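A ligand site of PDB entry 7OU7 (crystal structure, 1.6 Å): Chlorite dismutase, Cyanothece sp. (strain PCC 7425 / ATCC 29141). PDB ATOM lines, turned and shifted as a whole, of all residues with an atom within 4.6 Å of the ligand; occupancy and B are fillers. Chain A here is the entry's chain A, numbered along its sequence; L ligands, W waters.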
ATOM      1  N   ASN A  64      25.359  14.044  -8.173  1.00  0.00           N
ATOM      2  CA  ASN A  64      25.321  14.045  -9.616  1.00  0.00           C
ATOM      3  C   ASN A  64      25.700  12.678 -10.191  1.00  0.00           C
ATOM      4  O   ASN A  64      26.311  11.827  -9.516  1.00  0.00           O
ATOM      5  CB  ASN A  64      26.278  15.103 -10.197  1.00  0.00           C
ATOM      6  CG  ASN A  64      27.717  14.866  -9.790  1.00  0.00           C
ATOM      7  OD1 ASN A  64      28.102  15.198  -8.676  1.00  0.00           O
ATOM      8  ND2 ASN A  64      28.529  14.310 -10.707  1.00  0.00           N
ATOM      9  N   ILE A  65      25.308  12.489 -11.448  1.00  0.00           N
ATOM     10  CA  ILE A  65      25.631  11.276 -12.196  1.00  0.00           C
ATOM     11  C   ILE A  65      27.148  11.125 -12.337  1.00  0.00           C
ATOM     12  O   ILE A  65      27.861  12.087 -12.645  1.00  0.00           O
ATOM     13  CB  ILE A  65      24.949  11.333 -13.575  1.00  0.00           C
ATOM     14  CG1 ILE A  65      23.439  11.100 -13.435  1.00  0.00           C
ATOM     15  CG2 ILE A  65      25.595  10.345 -14.558  1.00  0.00           C
ATOM     16  CD1 ILE A  65      23.081   9.697 -12.952  1.00  0.00           C
ATOM     17  N   ARG A  66      27.630   9.889 -12.108  1.00  0.00           N
ATOM     18  CA  ARG A  66      29.066   9.590 -12.175  1.00  0.00           C
ATOM     19  C   ARG A  66      29.481   8.710 -13.346  1.00  0.00           C
ATOM     20  O   ARG A  66      30.674   8.712 -13.705  1.00  0.00           O
ATOM     21  CB  ARG A  66      29.516   8.873 -10.887  1.00  0.00           C
ATOM     22  CG  ARG A  66      29.052   9.526  -9.588  1.00  0.00           C
ATOM     23  CD  ARG A  66      29.522  10.989  -9.522  1.00  0.00           C
ATOM     24  NE  ARG A  66      29.121  11.613  -8.269  1.00  0.00           N
ATOM     25  CZ  ARG A  66      29.767  11.463  -7.112  1.00  0.00           C
ATOM     26  NH1 ARG A  66      30.860  10.712  -7.028  1.00  0.00           N
ATOM     27  NH2 ARG A  66      29.303  12.072  -6.022  1.00  0.00           N
ATOM     28  N   TYR A  67      28.545   7.941 -13.926  1.00  0.00           N
ATOM     29  CA  TYR A  67      28.881   6.968 -14.969  1.00  0.00           C
ATOM     30  C   TYR A  67      27.910   6.965 -16.149  1.00  0.00           C
ATOM     31  O   TYR A  67      28.333   6.788 -17.289  1.00  0.00           O
ATOM     32  CB  TYR A  67      28.947   5.540 -14.393  1.00  0.00           C
ATOM     33  CG  TYR A  67      30.049   5.372 -13.364  1.00  0.00           C
ATOM     34  CD1 TYR A  67      31.382   5.429 -13.741  1.00  0.00           C
ATOM     35  CD2 TYR A  67      29.746   5.163 -12.024  1.00  0.00           C
ATOM     36  CE1 TYR A  67      32.389   5.295 -12.802  1.00  0.00           C
ATOM     37  CE2 TYR A  67      30.765   5.018 -11.080  1.00  0.00           C
ATOM     38  CZ  TYR A  67      32.080   5.087 -11.486  1.00  0.00           C
ATOM     39  OH  TYR A  67      33.100   4.955 -10.558  1.00  0.00           O
ATOM     40  N   ALA A  68      26.611   7.141 -15.883  1.00  0.00           N
ATOM     41  CA  ALA A  68      25.610   6.977 -16.922  1.00  0.00           C
ATOM     42  C   ALA A  68      25.806   8.001 -18.024  1.00  0.00           C
ATOM     43  O   ALA A  68      26.076   9.176 -17.755  1.00  0.00           O
ATOM     44  CB  ALA A  68      24.194   7.100 -16.336  1.00  0.00           C
ATOM     45  N   LEU A  76      16.643   5.595 -18.371  1.00  0.00           N
ATOM     46  CA  LEU A  76      16.339   5.453 -16.943  1.00  0.00           C
ATOM     47  C   LEU A  76      15.250   6.420 -16.524  1.00  0.00           C
ATOM     48  O   LEU A  76      14.234   6.023 -15.934  1.00  0.00           O
ATOM     49  CB  LEU A  76      17.604   5.705 -16.120  1.00  0.00           C
ATOM     50  CG  LEU A  76      18.723   4.679 -16.243  1.00  0.00           C
ATOM     51  CD1 LEU A  76      20.081   5.360 -16.133  1.00  0.00           C
ATOM     52  CD2 LEU A  76      18.568   3.616 -15.170  1.00  0.00           C
ATOM     53  N   ILE A  94      20.071  -1.505   0.700  1.00  0.00           N
ATOM     54  CA  ILE A  94      21.285  -2.301   0.528  1.00  0.00           C
ATOM     55  C   ILE A  94      22.516  -1.408   0.631  1.00  0.00           C
ATOM     56  O   ILE A  94      22.944  -0.812  -0.375  1.00  0.00           O
ATOM     57  CB  ILE A  94      21.282  -3.098  -0.791  1.00  0.00           C
ATOM     58  CG1 ILE A  94      19.983  -3.880  -0.926  1.00  0.00           C
ATOM     59  CG2 ILE A  94      22.482  -4.060  -0.840  1.00  0.00           C
ATOM     60  CD1 ILE A  94      19.871  -4.705  -2.206  1.00  0.00           C
ATOM     61  N   ILE A  96      26.409  -0.711   0.625  1.00  0.00           N
ATOM     62  CA  ILE A  96      27.476  -1.365  -0.121  1.00  0.00           C
ATOM     63  C   ILE A  96      28.780  -0.614   0.077  1.00  0.00           C
ATOM     64  O   ILE A  96      28.809   0.622   0.035  1.00  0.00           O
ATOM     65  CB  ILE A  96      27.114  -1.449  -1.624  1.00  0.00           C
ATOM     66  CG1 ILE A  96      26.050  -2.538  -1.822  1.00  0.00           C
ATOM     67  CG2 ILE A  96      28.338  -1.736  -2.490  1.00  0.00           C
ATOM     68  CD1 ILE A  96      25.323  -2.415  -3.140  1.00  0.00           C
ATOM     69  N   LYS A  98      32.802  -0.616  -1.510  1.00  0.00           N
ATOM     70  CA  LYS A  98      33.730  -1.153  -2.484  1.00  0.00           C
ATOM     71  C   LYS A  98      35.164  -1.025  -1.977  1.00  0.00           C
ATOM     72  O   LYS A  98      35.467  -0.247  -1.066  1.00  0.00           O
ATOM     73  CB  LYS A  98      33.572  -0.456  -3.843  1.00  0.00           C
ATOM     74  CG  LYS A  98      32.223  -0.769  -4.513  1.00  0.00           C
ATOM     75  CD  LYS A  98      32.126  -0.138  -5.907  1.00  0.00           C
ATOM     76  CE  LYS A  98      30.815  -0.569  -6.591  1.00  0.00           C
ATOM     77  NZ  LYS A  98      30.725  -0.008  -7.975  1.00  0.00           N
ATOM     78  N   TRP A 102      39.152  -0.552  -6.016  1.00  0.00           N
ATOM     79  CA  TRP A 102      38.175   0.105  -6.884  1.00  0.00           C
ATOM     80  C   TRP A 102      38.421   1.612  -6.916  1.00  0.00           C
ATOM     81  O   TRP A 102      38.523   2.216  -7.999  1.00  0.00           O
ATOM     82  CB  TRP A 102      36.770  -0.182  -6.370  1.00  0.00           C
ATOM     83  CG  TRP A 102      35.719   0.613  -7.059  1.00  0.00           C
ATOM     84  CD1 TRP A 102      35.123   1.758  -6.595  1.00  0.00           C
ATOM     85  CD2 TRP A 102      35.102   0.322  -8.324  1.00  0.00           C
ATOM     86  NE1 TRP A 102      34.207   2.209  -7.505  1.00  0.00           N
ATOM     87  CE2 TRP A 102      34.160   1.343  -8.564  1.00  0.00           C
ATOM     88  CE3 TRP A 102      35.266  -0.706  -9.262  1.00  0.00           C
ATOM     89  CZ2 TRP A 102      33.368   1.367  -9.719  1.00  0.00           C
ATOM     90  CZ3 TRP A 102      34.480  -0.665 -10.417  1.00  0.00           C
ATOM     91  CH2 TRP A 102      33.553   0.357 -10.631  1.00  0.00           C
ATOM     92  N   PHE A 114      31.895  -1.030 -14.670  1.00  0.00           N
ATOM     93  CA  PHE A 114      30.503  -0.789 -14.282  1.00  0.00           C
ATOM     94  C   PHE A 114      29.536  -1.137 -15.410  1.00  0.00           C
ATOM     95  O   PHE A 114      28.505  -1.788 -15.188  1.00  0.00           O
ATOM     96  CB  PHE A 114      30.346   0.670 -13.846  1.00  0.00           C
ATOM     97  CG  PHE A 114      28.944   1.081 -13.530  1.00  0.00           C
ATOM     98  CD1 PHE A 114      28.396   0.799 -12.288  1.00  0.00           C
ATOM     99  CD2 PHE A 114      28.184   1.776 -14.452  1.00  0.00           C
ATOM    100  CE1 PHE A 114      27.103   1.177 -11.983  1.00  0.00           C
ATOM    101  CE2 PHE A 114      26.868   2.161 -14.154  1.00  0.00           C
ATOM    102  CZ  PHE A 114      26.331   1.851 -12.921  1.00  0.00           C
ATOM    103  N   HIS A 120      25.621  -2.932 -15.722  1.00  0.00           N
ATOM    104  CA  HIS A 120      24.800  -2.538 -14.577  1.00  0.00           C
ATOM    105  C   HIS A 120      23.515  -1.860 -15.009  1.00  0.00           C
ATOM    106  O   HIS A 120      22.404  -2.266 -14.629  1.00  0.00           O
ATOM    107  CB  HIS A 120      25.605  -1.628 -13.642  1.00  0.00           C
ATOM    108  CG  HIS A 120      24.931  -1.317 -12.343  1.00  0.00           C
ATOM    109  ND1 HIS A 120      25.469  -1.660 -11.122  1.00  0.00           N
ATOM    110  CD2 HIS A 120      23.771  -0.675 -12.073  1.00  0.00           C
ATOM    111  CE1 HIS A 120      24.670  -1.232 -10.152  1.00  0.00           C
ATOM    112  NE2 HIS A 120      23.615  -0.650 -10.702  1.00  0.00           N
ATOM    113  N   THR A 121      23.640  -0.803 -15.824  1.00  0.00           N
ATOM    114  CA  THR A 121      22.457  -0.045 -16.244  1.00  0.00           C
ATOM    115  C   THR A 121      21.593  -0.841 -17.207  1.00  0.00           C
ATOM    116  O   THR A 121      20.366  -0.857 -17.085  1.00  0.00           O
ATOM    117  CB  THR A 121      22.912   1.268 -16.883  1.00  0.00           C
ATOM    118  OG1 THR A 121      23.808   1.948 -15.995  1.00  0.00           O
ATOM    119  CG2 THR A 121      21.731   2.149 -17.197  1.00  0.00           C
ATOM    120  N   GLY A 124      19.845  -3.522 -15.214  1.00  0.00           N
ATOM    121  CA  GLY A 124      18.895  -2.885 -14.316  1.00  0.00           C
ATOM    122  C   GLY A 124      17.660  -2.386 -15.033  1.00  0.00           C
ATOM    123  O   GLY A 124      16.537  -2.474 -14.512  1.00  0.00           O
ATOM    124  N   LEU A 125      17.822  -1.842 -16.248  1.00  0.00           N
ATOM    125  CA  LEU A 125      16.677  -1.295 -16.953  1.00  0.00           C
ATOM    126  C   LEU A 125      15.620  -2.362 -17.248  1.00  0.00           C
ATOM    127  O   LEU A 125      14.443  -2.029 -17.399  1.00  0.00           O
ATOM    128  CB  LEU A 125      17.121  -0.620 -18.251  1.00  0.00           C
ATOM    129  CG  LEU A 125      17.786   0.749 -18.076  1.00  0.00           C
ATOM    130  CD1 LEU A 125      18.515   1.161 -19.340  1.00  0.00           C
ATOM    131  CD2 LEU A 125      16.728   1.791 -17.701  1.00  0.00           C
ATOM    132  N   LEU A 128      13.663  -2.187 -13.999  1.00  0.00           N
ATOM    133  CA  LEU A 128      13.304  -0.882 -13.470  1.00  0.00           C
ATOM    134  C   LEU A 128      11.815  -0.527 -13.601  1.00  0.00           C
ATOM    135  O   LEU A 128      11.316   0.191 -12.717  1.00  0.00           O
ATOM    136  CB  LEU A 128      14.158   0.182 -14.162  1.00  0.00           C
ATOM    137  CG  LEU A 128      14.192   1.554 -13.486  1.00  0.00           C
ATOM    138  CD1 LEU A 128      14.830   1.464 -12.109  1.00  0.00           C
ATOM    139  CD2 LEU A 128      14.969   2.497 -14.372  1.00  0.00           C
ATOM    140  N   VAL A 131      10.289  -1.109 -10.314  1.00  0.00           N
ATOM    141  CA  VAL A 131      11.137  -0.902  -9.145  1.00  0.00           C
ATOM    142  C   VAL A 131      11.528   0.566  -9.065  1.00  0.00           C
ATOM    143  O   VAL A 131      12.209   1.077  -9.954  1.00  0.00           O
ATOM    144  CB  VAL A 131      12.392  -1.798  -9.192  1.00  0.00           C
ATOM    145  CG1 VAL A 131      13.303  -1.503  -7.993  1.00  0.00           C
ATOM    146  CG2 VAL A 131      12.001  -3.259  -9.192  1.00  0.00           C
ATOM    147  N   ARG A 133      13.834   3.404  -7.374  1.00  0.00           N
ATOM    148  CA  ARG A 133      15.198   3.293  -6.861  1.00  0.00           C
ATOM    149  C   ARG A 133      15.732   4.661  -6.465  1.00  0.00           C
ATOM    150  O   ARG A 133      15.416   5.669  -7.088  1.00  0.00           O
ATOM    151  CB  ARG A 133      16.126   2.627  -7.896  1.00  0.00           C
ATOM    152  CG  ARG A 133      16.720   3.556  -8.935  1.00  0.00           C
ATOM    153  CD  ARG A 133      17.684   2.853  -9.896  1.00  0.00           C
ATOM    154  NE  ARG A 133      19.068   3.176  -9.593  1.00  0.00           N
ATOM    155  CZ  ARG A 133      19.647   4.321  -9.929  1.00  0.00           C
ATOM    156  NH1 ARG A 133      18.988   5.270 -10.569  1.00  0.00           N
ATOM    157  NH2 ARG A 133      20.928   4.534  -9.599  1.00  0.00           N
ATOM    158  N   LEU A 135      19.674   6.112  -5.246  1.00  0.00           N
ATOM    159  CA  LEU A 135      21.097   5.911  -4.950  1.00  0.00           C
ATOM    160  C   LEU A 135      21.628   7.073  -4.119  1.00  0.00           C
ATOM    161  O   LEU A 135      21.474   8.233  -4.499  1.00  0.00           O
ATOM    162  CB  LEU A 135      21.892   5.808  -6.251  1.00  0.00           C
ATOM    163  CG  LEU A 135      23.408   5.788  -6.067  1.00  0.00           C
ATOM    164  CD1 LEU A 135      23.868   4.482  -5.452  1.00  0.00           C
ATOM    165  CD2 LEU A 135      24.085   6.016  -7.422  1.00  0.00           C
ATOM    166  N   PHE A 147      27.933   3.412  -0.344  1.00  0.00           N
ATOM    167  CA  PHE A 147      26.664   3.740  -0.979  1.00  0.00           C
ATOM    168  C   PHE A 147      25.539   3.205  -0.131  1.00  0.00           C
ATOM    169  O   PHE A 147      25.683   2.204   0.570  1.00  0.00           O
ATOM    170  CB  PHE A 147      26.543   3.127  -2.387  1.00  0.00           C
ATOM    171  CG  PHE A 147      27.696   3.430  -3.284  1.00  0.00           C
ATOM    172  CD1 PHE A 147      27.735   4.635  -3.977  1.00  0.00           C
ATOM    173  CD2 PHE A 147      28.719   2.518  -3.461  1.00  0.00           C
ATOM    174  CE1 PHE A 147      28.794   4.917  -4.817  1.00  0.00           C
ATOM    175  CE2 PHE A 147      29.759   2.795  -4.306  1.00  0.00           C
ATOM    176  CZ  PHE A 147      29.795   3.996  -4.977  1.00  0.00           C
ATOM    177  N   THR A 149      21.757   2.071  -1.206  1.00  0.00           N
ATOM    178  CA  THR A 149      20.845   1.887  -2.321  1.00  0.00           C
ATOM    179  C   THR A 149      19.473   1.502  -1.779  1.00  0.00           C
ATOM    180  O   THR A 149      19.371   0.806  -0.753  1.00  0.00           O
ATOM    181  CB  THR A 149      21.355   0.832  -3.321  1.00  0.00           C
ATOM    182  OG1 THR A 149      21.448  -0.464  -2.707  1.00  0.00           O
ATOM    183  CG2 THR A 149      22.736   1.220  -3.860  1.00  0.00           C
ATOM    184  N   PHE A 151      15.388   0.398  -2.876  1.00  0.00           N
ATOM    185  CA  PHE A 151      14.500  -0.114  -3.913  1.00  0.00           C
ATOM    186  C   PHE A 151      13.150  -0.396  -3.280  1.00  0.00           C
ATOM    187  O   PHE A 151      13.076  -0.905  -2.162  1.00  0.00           O
ATOM    188  CB  PHE A 151      15.079  -1.389  -4.538  1.00  0.00           C
ATOM    189  CG  PHE A 151      16.481  -1.217  -4.990  1.00  0.00           C
ATOM    190  CD1 PHE A 151      16.763  -0.636  -6.212  1.00  0.00           C
ATOM    191  CD2 PHE A 151      17.529  -1.556  -4.143  1.00  0.00           C
ATOM    192  CE1 PHE A 151      18.076  -0.432  -6.603  1.00  0.00           C
ATOM    193  CE2 PHE A 151      18.842  -1.358  -4.526  1.00  0.00           C
ATOM    194  CZ  PHE A 151      19.117  -0.805  -5.769  1.00  0.00           C
ATOM    195  N   PHE A 161      12.962  -9.173  -8.354  1.00  0.00           N
ATOM    196  CA  PHE A 161      14.057  -8.450  -7.717  1.00  0.00           C
ATOM    197  C   PHE A 161      15.145  -9.406  -7.237  1.00  0.00           C
ATOM    198  O   PHE A 161      16.344  -9.104  -7.330  1.00  0.00           O
ATOM    199  CB  PHE A 161      13.537  -7.593  -6.566  1.00  0.00           C
ATOM    200  CG  PHE A 161      14.558  -6.641  -6.033  1.00  0.00           C
ATOM    201  CD1 PHE A 161      14.864  -5.477  -6.713  1.00  0.00           C
ATOM    202  CD2 PHE A 161      15.249  -6.941  -4.877  1.00  0.00           C
ATOM    203  CE1 PHE A 161      15.839  -4.618  -6.227  1.00  0.00           C
ATOM    204  CE2 PHE A 161      16.215  -6.086  -4.394  1.00  0.00           C
ATOM    205  CZ  PHE A 161      16.512  -4.931  -5.068  1.00  0.00           C
ATOM    206  N   LEU A 164      17.255 -10.189 -10.164  1.00  0.00           N
ATOM    207  CA  LEU A 164      18.208  -9.117 -10.445  1.00  0.00           C
ATOM    208  C   LEU A 164      19.420  -9.208  -9.519  1.00  0.00           C
ATOM    209  O   LEU A 164      20.566  -9.054  -9.952  1.00  0.00           O
ATOM    210  CB  LEU A 164      17.513  -7.765 -10.304  1.00  0.00           C
ATOM    211  CG  LEU A 164      18.422  -6.541 -10.333  1.00  0.00           C
ATOM    212  CD1 LEU A 164      19.132  -6.454 -11.693  1.00  0.00           C
ATOM    213  CD2 LEU A 164      17.631  -5.283 -10.039  1.00  0.00           C
ATOM    214  N   LEU A 165      19.177  -9.471  -8.231  1.00  0.00           N
ATOM    215  CA  LEU A 165      20.294  -9.583  -7.285  1.00  0.00           C
ATOM    216  C   LEU A 165      21.212 -10.734  -7.658  1.00  0.00           C
ATOM    217  O   LEU A 165      22.443 -10.626  -7.560  1.00  0.00           O
ATOM    218  CB  LEU A 165      19.776  -9.764  -5.854  1.00  0.00           C
ATOM    219  CG  LEU A 165      19.070  -8.584  -5.202  1.00  0.00           C
ATOM    220  CD1 LEU A 165      18.591  -8.976  -3.804  1.00  0.00           C
ATOM    221  CD2 LEU A 165      20.010  -7.402  -5.137  1.00  0.00           C
ATOM    222  N   MET A 168      23.379  -9.430 -10.547  1.00  0.00           N
ATOM    223  CA  MET A 168      24.392  -8.414 -10.230  1.00  0.00           C
ATOM    224  C   MET A 168      25.503  -8.979  -9.363  1.00  0.00           C
ATOM    225  O   MET A 168      26.674  -8.599  -9.525  1.00  0.00           O
ATOM    226  CB  MET A 168      23.761  -7.188  -9.592  1.00  0.00           C
ATOM    227  CG  MET A 168      22.601  -6.649 -10.403  1.00  0.00           C
ATOM    228  SD  MET A 168      21.971  -5.086  -9.786  1.00  0.00           S
ATOM    229  CE  MET A 168      23.497  -4.181  -9.453  1.00  0.00           C
ATOM    230  N   GLU A 173      31.737  -6.100 -11.601  1.00  0.00           N
ATOM    231  CA  GLU A 173      31.678  -5.012 -10.640  1.00  0.00           C
ATOM    232  C   GLU A 173      31.642  -5.546  -9.213  1.00  0.00           C
ATOM    233  O   GLU A 173      32.254  -4.978  -8.304  1.00  0.00           O
ATOM    234  CB  GLU A 173      30.444  -4.131 -10.918  1.00  0.00           C
ATOM    235  CG  GLU A 173      30.242  -3.015  -9.889  1.00  0.00           C
ATOM    236  CD  GLU A 173      28.948  -2.228 -10.115  1.00  0.00           C
ATOM    237  OE1 GLU A 173      28.123  -2.633 -10.968  1.00  0.00           O
ATOM    238  OE2 GLU A 173      28.770  -1.185  -9.441  1.00  0.00           O
ATOM    239  N   TRP A 174      30.884  -6.621  -8.980  1.00  0.00           N
ATOM    240  CA  TRP A 174      30.753  -7.139  -7.618  1.00  0.00           C
ATOM    241  C   TRP A 174      32.026  -7.788  -7.089  1.00  0.00           C
ATOM    242  O   TRP A 174      32.115  -8.018  -5.880  1.00  0.00           O
ATOM    243  CB  TRP A 174      29.584  -8.128  -7.517  1.00  0.00           C
ATOM    244  CG  TRP A 174      28.520  -7.567  -6.628  1.00  0.00           C
ATOM    245  CD1 TRP A 174      28.214  -7.967  -5.357  1.00  0.00           C
ATOM    246  CD2 TRP A 174      27.679  -6.447  -6.916  1.00  0.00           C
ATOM    247  NE1 TRP A 174      27.212  -7.184  -4.851  1.00  0.00           N
ATOM    248  CE2 TRP A 174      26.863  -6.245  -5.779  1.00  0.00           C
ATOM    249  CE3 TRP A 174      27.516  -5.619  -8.024  1.00  0.00           C
ATOM    250  CZ2 TRP A 174      25.915  -5.232  -5.724  1.00  0.00           C
ATOM    251  CZ3 TRP A 174      26.568  -4.606  -7.970  1.00  0.00           C
ATOM    252  CH2 TRP A 174      25.778  -4.419  -6.831  1.00  0.00           C
ATOM    253  N   GLU A 180      28.454  -5.762   2.280  1.00  0.00           N
ATOM    254  CA  GLU A 180      27.114  -5.659   1.723  1.00  0.00           C
ATOM    255  C   GLU A 180      26.135  -6.234   2.720  1.00  0.00           C
ATOM    256  O   GLU A 180      26.360  -7.326   3.253  1.00  0.00           O
ATOM    257  CB  GLU A 180      27.016  -6.403   0.379  1.00  0.00           C
ATOM    258  CG  GLU A 180      25.662  -6.253  -0.305  1.00  0.00           C
ATOM    259  CD  GLU A 180      25.629  -6.837  -1.714  1.00  0.00           C
ATOM    260  OE1 GLU A 180      26.606  -7.499  -2.130  1.00  0.00           O
ATOM    261  OE2 GLU A 180      24.628  -6.588  -2.428  1.00  0.00           O
HETATM  262  C1  LIG L   1      24.762   2.931  -9.467  1.00  0.00           C
HETATM  263  C2  LIG L   1      20.999   1.777 -12.314  1.00  0.00           C
HETATM  264  C3  LIG L   1      19.864  -1.877  -9.337  1.00  0.00           C
HETATM  265  C4  LIG L   1      23.796  -0.888  -6.624  1.00  0.00           C
HETATM  266  C5  LIG L   1      23.855   2.918 -10.503  1.00  0.00           C
HETATM  267  C6  LIG L   1      23.859   3.820 -11.638  1.00  0.00           C
HETATM  268  C7  LIG L   1      22.832   3.495 -12.424  1.00  0.00           C
HETATM  269  C8  LIG L   1      22.125   2.397 -11.805  1.00  0.00           C
HETATM  270  C9  LIG L   1      22.445   4.176 -13.749  1.00  0.00           C
HETATM  271  C10 LIG L   1      24.903   4.915 -11.926  1.00  0.00           C
HETATM  272  C11 LIG L   1      24.495   6.281 -11.403  1.00  0.00           C
HETATM  273  C12 LIG L   1      25.593   7.238 -11.831  1.00  0.00           C
HETATM  274  O1  LIG L   1      26.165   7.919 -10.937  1.00  0.00           O
HETATM  275  O2  LIG L   1      25.922   7.268 -13.055  1.00  0.00           O
HETATM  276  C13 LIG L   1      20.354   0.730 -11.705  1.00  0.00           C
HETATM  277  C14 LIG L   1      19.094   0.190 -12.157  1.00  0.00           C
HETATM  278  C15 LIG L   1      18.755  -0.796 -11.343  1.00  0.00           C
HETATM  279  C16 LIG L   1      19.811  -0.959 -10.350  1.00  0.00           C
HETATM  280  C17 LIG L   1      18.306   0.746 -13.360  1.00  0.00           C
HETATM  281  C18 LIG L   1      17.453  -1.614 -11.467  1.00  0.00           C
HETATM  282  C19 LIG L   1      16.800  -1.913 -10.341  1.00  0.00           C
HETATM  283  C20 LIG L   1      20.852  -1.936  -8.367  1.00  0.00           C
HETATM  284  C21 LIG L   1      20.917  -2.925  -7.320  1.00  0.00           C
HETATM  285  C22 LIG L   1      21.988  -2.659  -6.553  1.00  0.00           C
HETATM  286  C23 LIG L   1      22.649  -1.494  -7.111  1.00  0.00           C
HETATM  287  C24 LIG L   1      19.888  -4.062  -7.127  1.00  0.00           C
HETATM  288  C25 LIG L   1      22.514  -3.409  -5.315  1.00  0.00           C
HETATM  289  C26 LIG L   1      22.256  -4.690  -5.074  1.00  0.00           C
HETATM  290  C27 LIG L   1      24.382   0.224  -7.161  1.00  0.00           C
HETATM  291  C28 LIG L   1      25.570   0.882  -6.646  1.00  0.00           C
HETATM  292  C29 LIG L   1      25.843   1.928  -7.440  1.00  0.00           C
HETATM  293  C30 LIG L   1      24.835   1.994  -8.469  1.00  0.00           C
HETATM  294  C31 LIG L   1      26.342   0.387  -5.409  1.00  0.00           C
HETATM  295  C32 LIG L   1      27.022   2.921  -7.288  1.00  0.00           C
HETATM  296  C33 LIG L   1      28.082   2.532  -8.322  1.00  0.00           C
HETATM  297  C34 LIG L   1      29.333   3.375  -8.193  1.00  0.00           C
HETATM  298  O3  LIG L   1      29.236   4.639  -8.192  1.00  0.00           O
HETATM  299  O4  LIG L   1      30.427   2.783  -8.089  1.00  0.00           O
HETATM  300  N1  LIG L   1      22.770   2.064 -10.636  1.00  0.00           N
HETATM  301  N2  LIG L   1      20.756   0.006 -10.600  1.00  0.00           N
HETATM  302  N3  LIG L   1      21.950  -1.086  -8.237  1.00  0.00           N
HETATM  303  N4  LIG L   1      23.975   0.937  -8.274  1.00  0.00           N
HETATM  304 FE1  LIG L   1      22.393   0.467  -9.458  1.00  0.00          FE
HETATM  305  O   HOH W   1      31.009   6.775  -7.485  1.00  0.00           O
HETATM  306  O   HOH W   2      32.432   4.403  -8.081  1.00  0.00           O
HETATM  307  O   HOH W   3      25.164   9.310  -8.841  1.00  0.00           O
HETATM  308  O   HOH W   4      27.287   6.250  -8.925  1.00  0.00           O
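The indole nitrogen (NE1) of Trp 174 is in hydrogen-bond range of the side-chain carboxylate (OE1) of Glu 180 (2.8 Å). O of Ile 96 lies within hydrogen-bond range of N of Phe 147 (2.9 Å). The backbone NH of His 120 sits at hydrogen-bond distance from the backbone carbonyl oxygen of Phe 114 (3.1 Å). OG1 of Thr 149 lies within hydrogen-bond range of O of Ile 94, 2.8 Å away. The guanidinium group of Arg 66 lies within hydrogen-bond range of the backbone carbonyl oxygen of Asn 64 (3.1 Å). NZ of Lys 98 lies within salt-bridge range of OE2 of Glu 173. A ring nitrogen (ND1) of His 120 lies within hydrogen-bond range of the side-chain carboxylate (OE1) of Glu 173 (2.8 Å).
The backbone NH of Tyr 67 lies within hydrogen-bond range of an oxygen (O2) of the ligand, 2.8 Å away. The backbone NH (N) of Ala 68 is in hydrogen-bond range of an oxygen (O2) of the ligand (2.9 Å). NE2 of His 120 binds FE1 of the ligand, at 2.1 Å. The backbone NH (N) of Arg 66 lies within hydrogen-bond range of an oxygen (O1) of the ligand (2.7 Å). NZ of Lys 98 is in salt-bridge range of O4 of the ligand, at 2.8 Å.
NH2 of Arg 133 sits close to N1 of the ligand (3.3 Å). Residues that only touch the ligand: Ile 65 (3.4 Å), Leu 76 (3.4 Å), Ile 94 (3.7 Å), Ile 96 (3.7 Å), Trp 102 (3.6 Å), Phe 114 (3.4 Å), Thr 121 (3.4 Å), Gly 124 (3.3 Å), Leu 125 (3.9 Å), Leu 128 (3.8 Å), Leu 135 (3.8 Å), Phe 147 (3.3 Å), Thr 149 (3.6 Å), Phe 151 (3.2 Å), Leu 164 (3.5 Å), Leu 165 (3.5 Å), Met 168 (3.4 Å), Glu 173 (3.9 Å) and Trp 174 (3.7 Å). Of the 29 residues printed, 25 come within 4 Å of the ligand.
Water W2 lies within hydrogen-bond range of an oxygen (O4) of the ligand (2.6 Å), the side-chain hydroxyl of Tyr 67 (2.6 Å) and the indole nitrogen of Trp 102 (2.9 Å). Water W3 bridges an oxygen (O1) of the ligand and the backbone carbonyl oxygen (O) of Asn 64.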
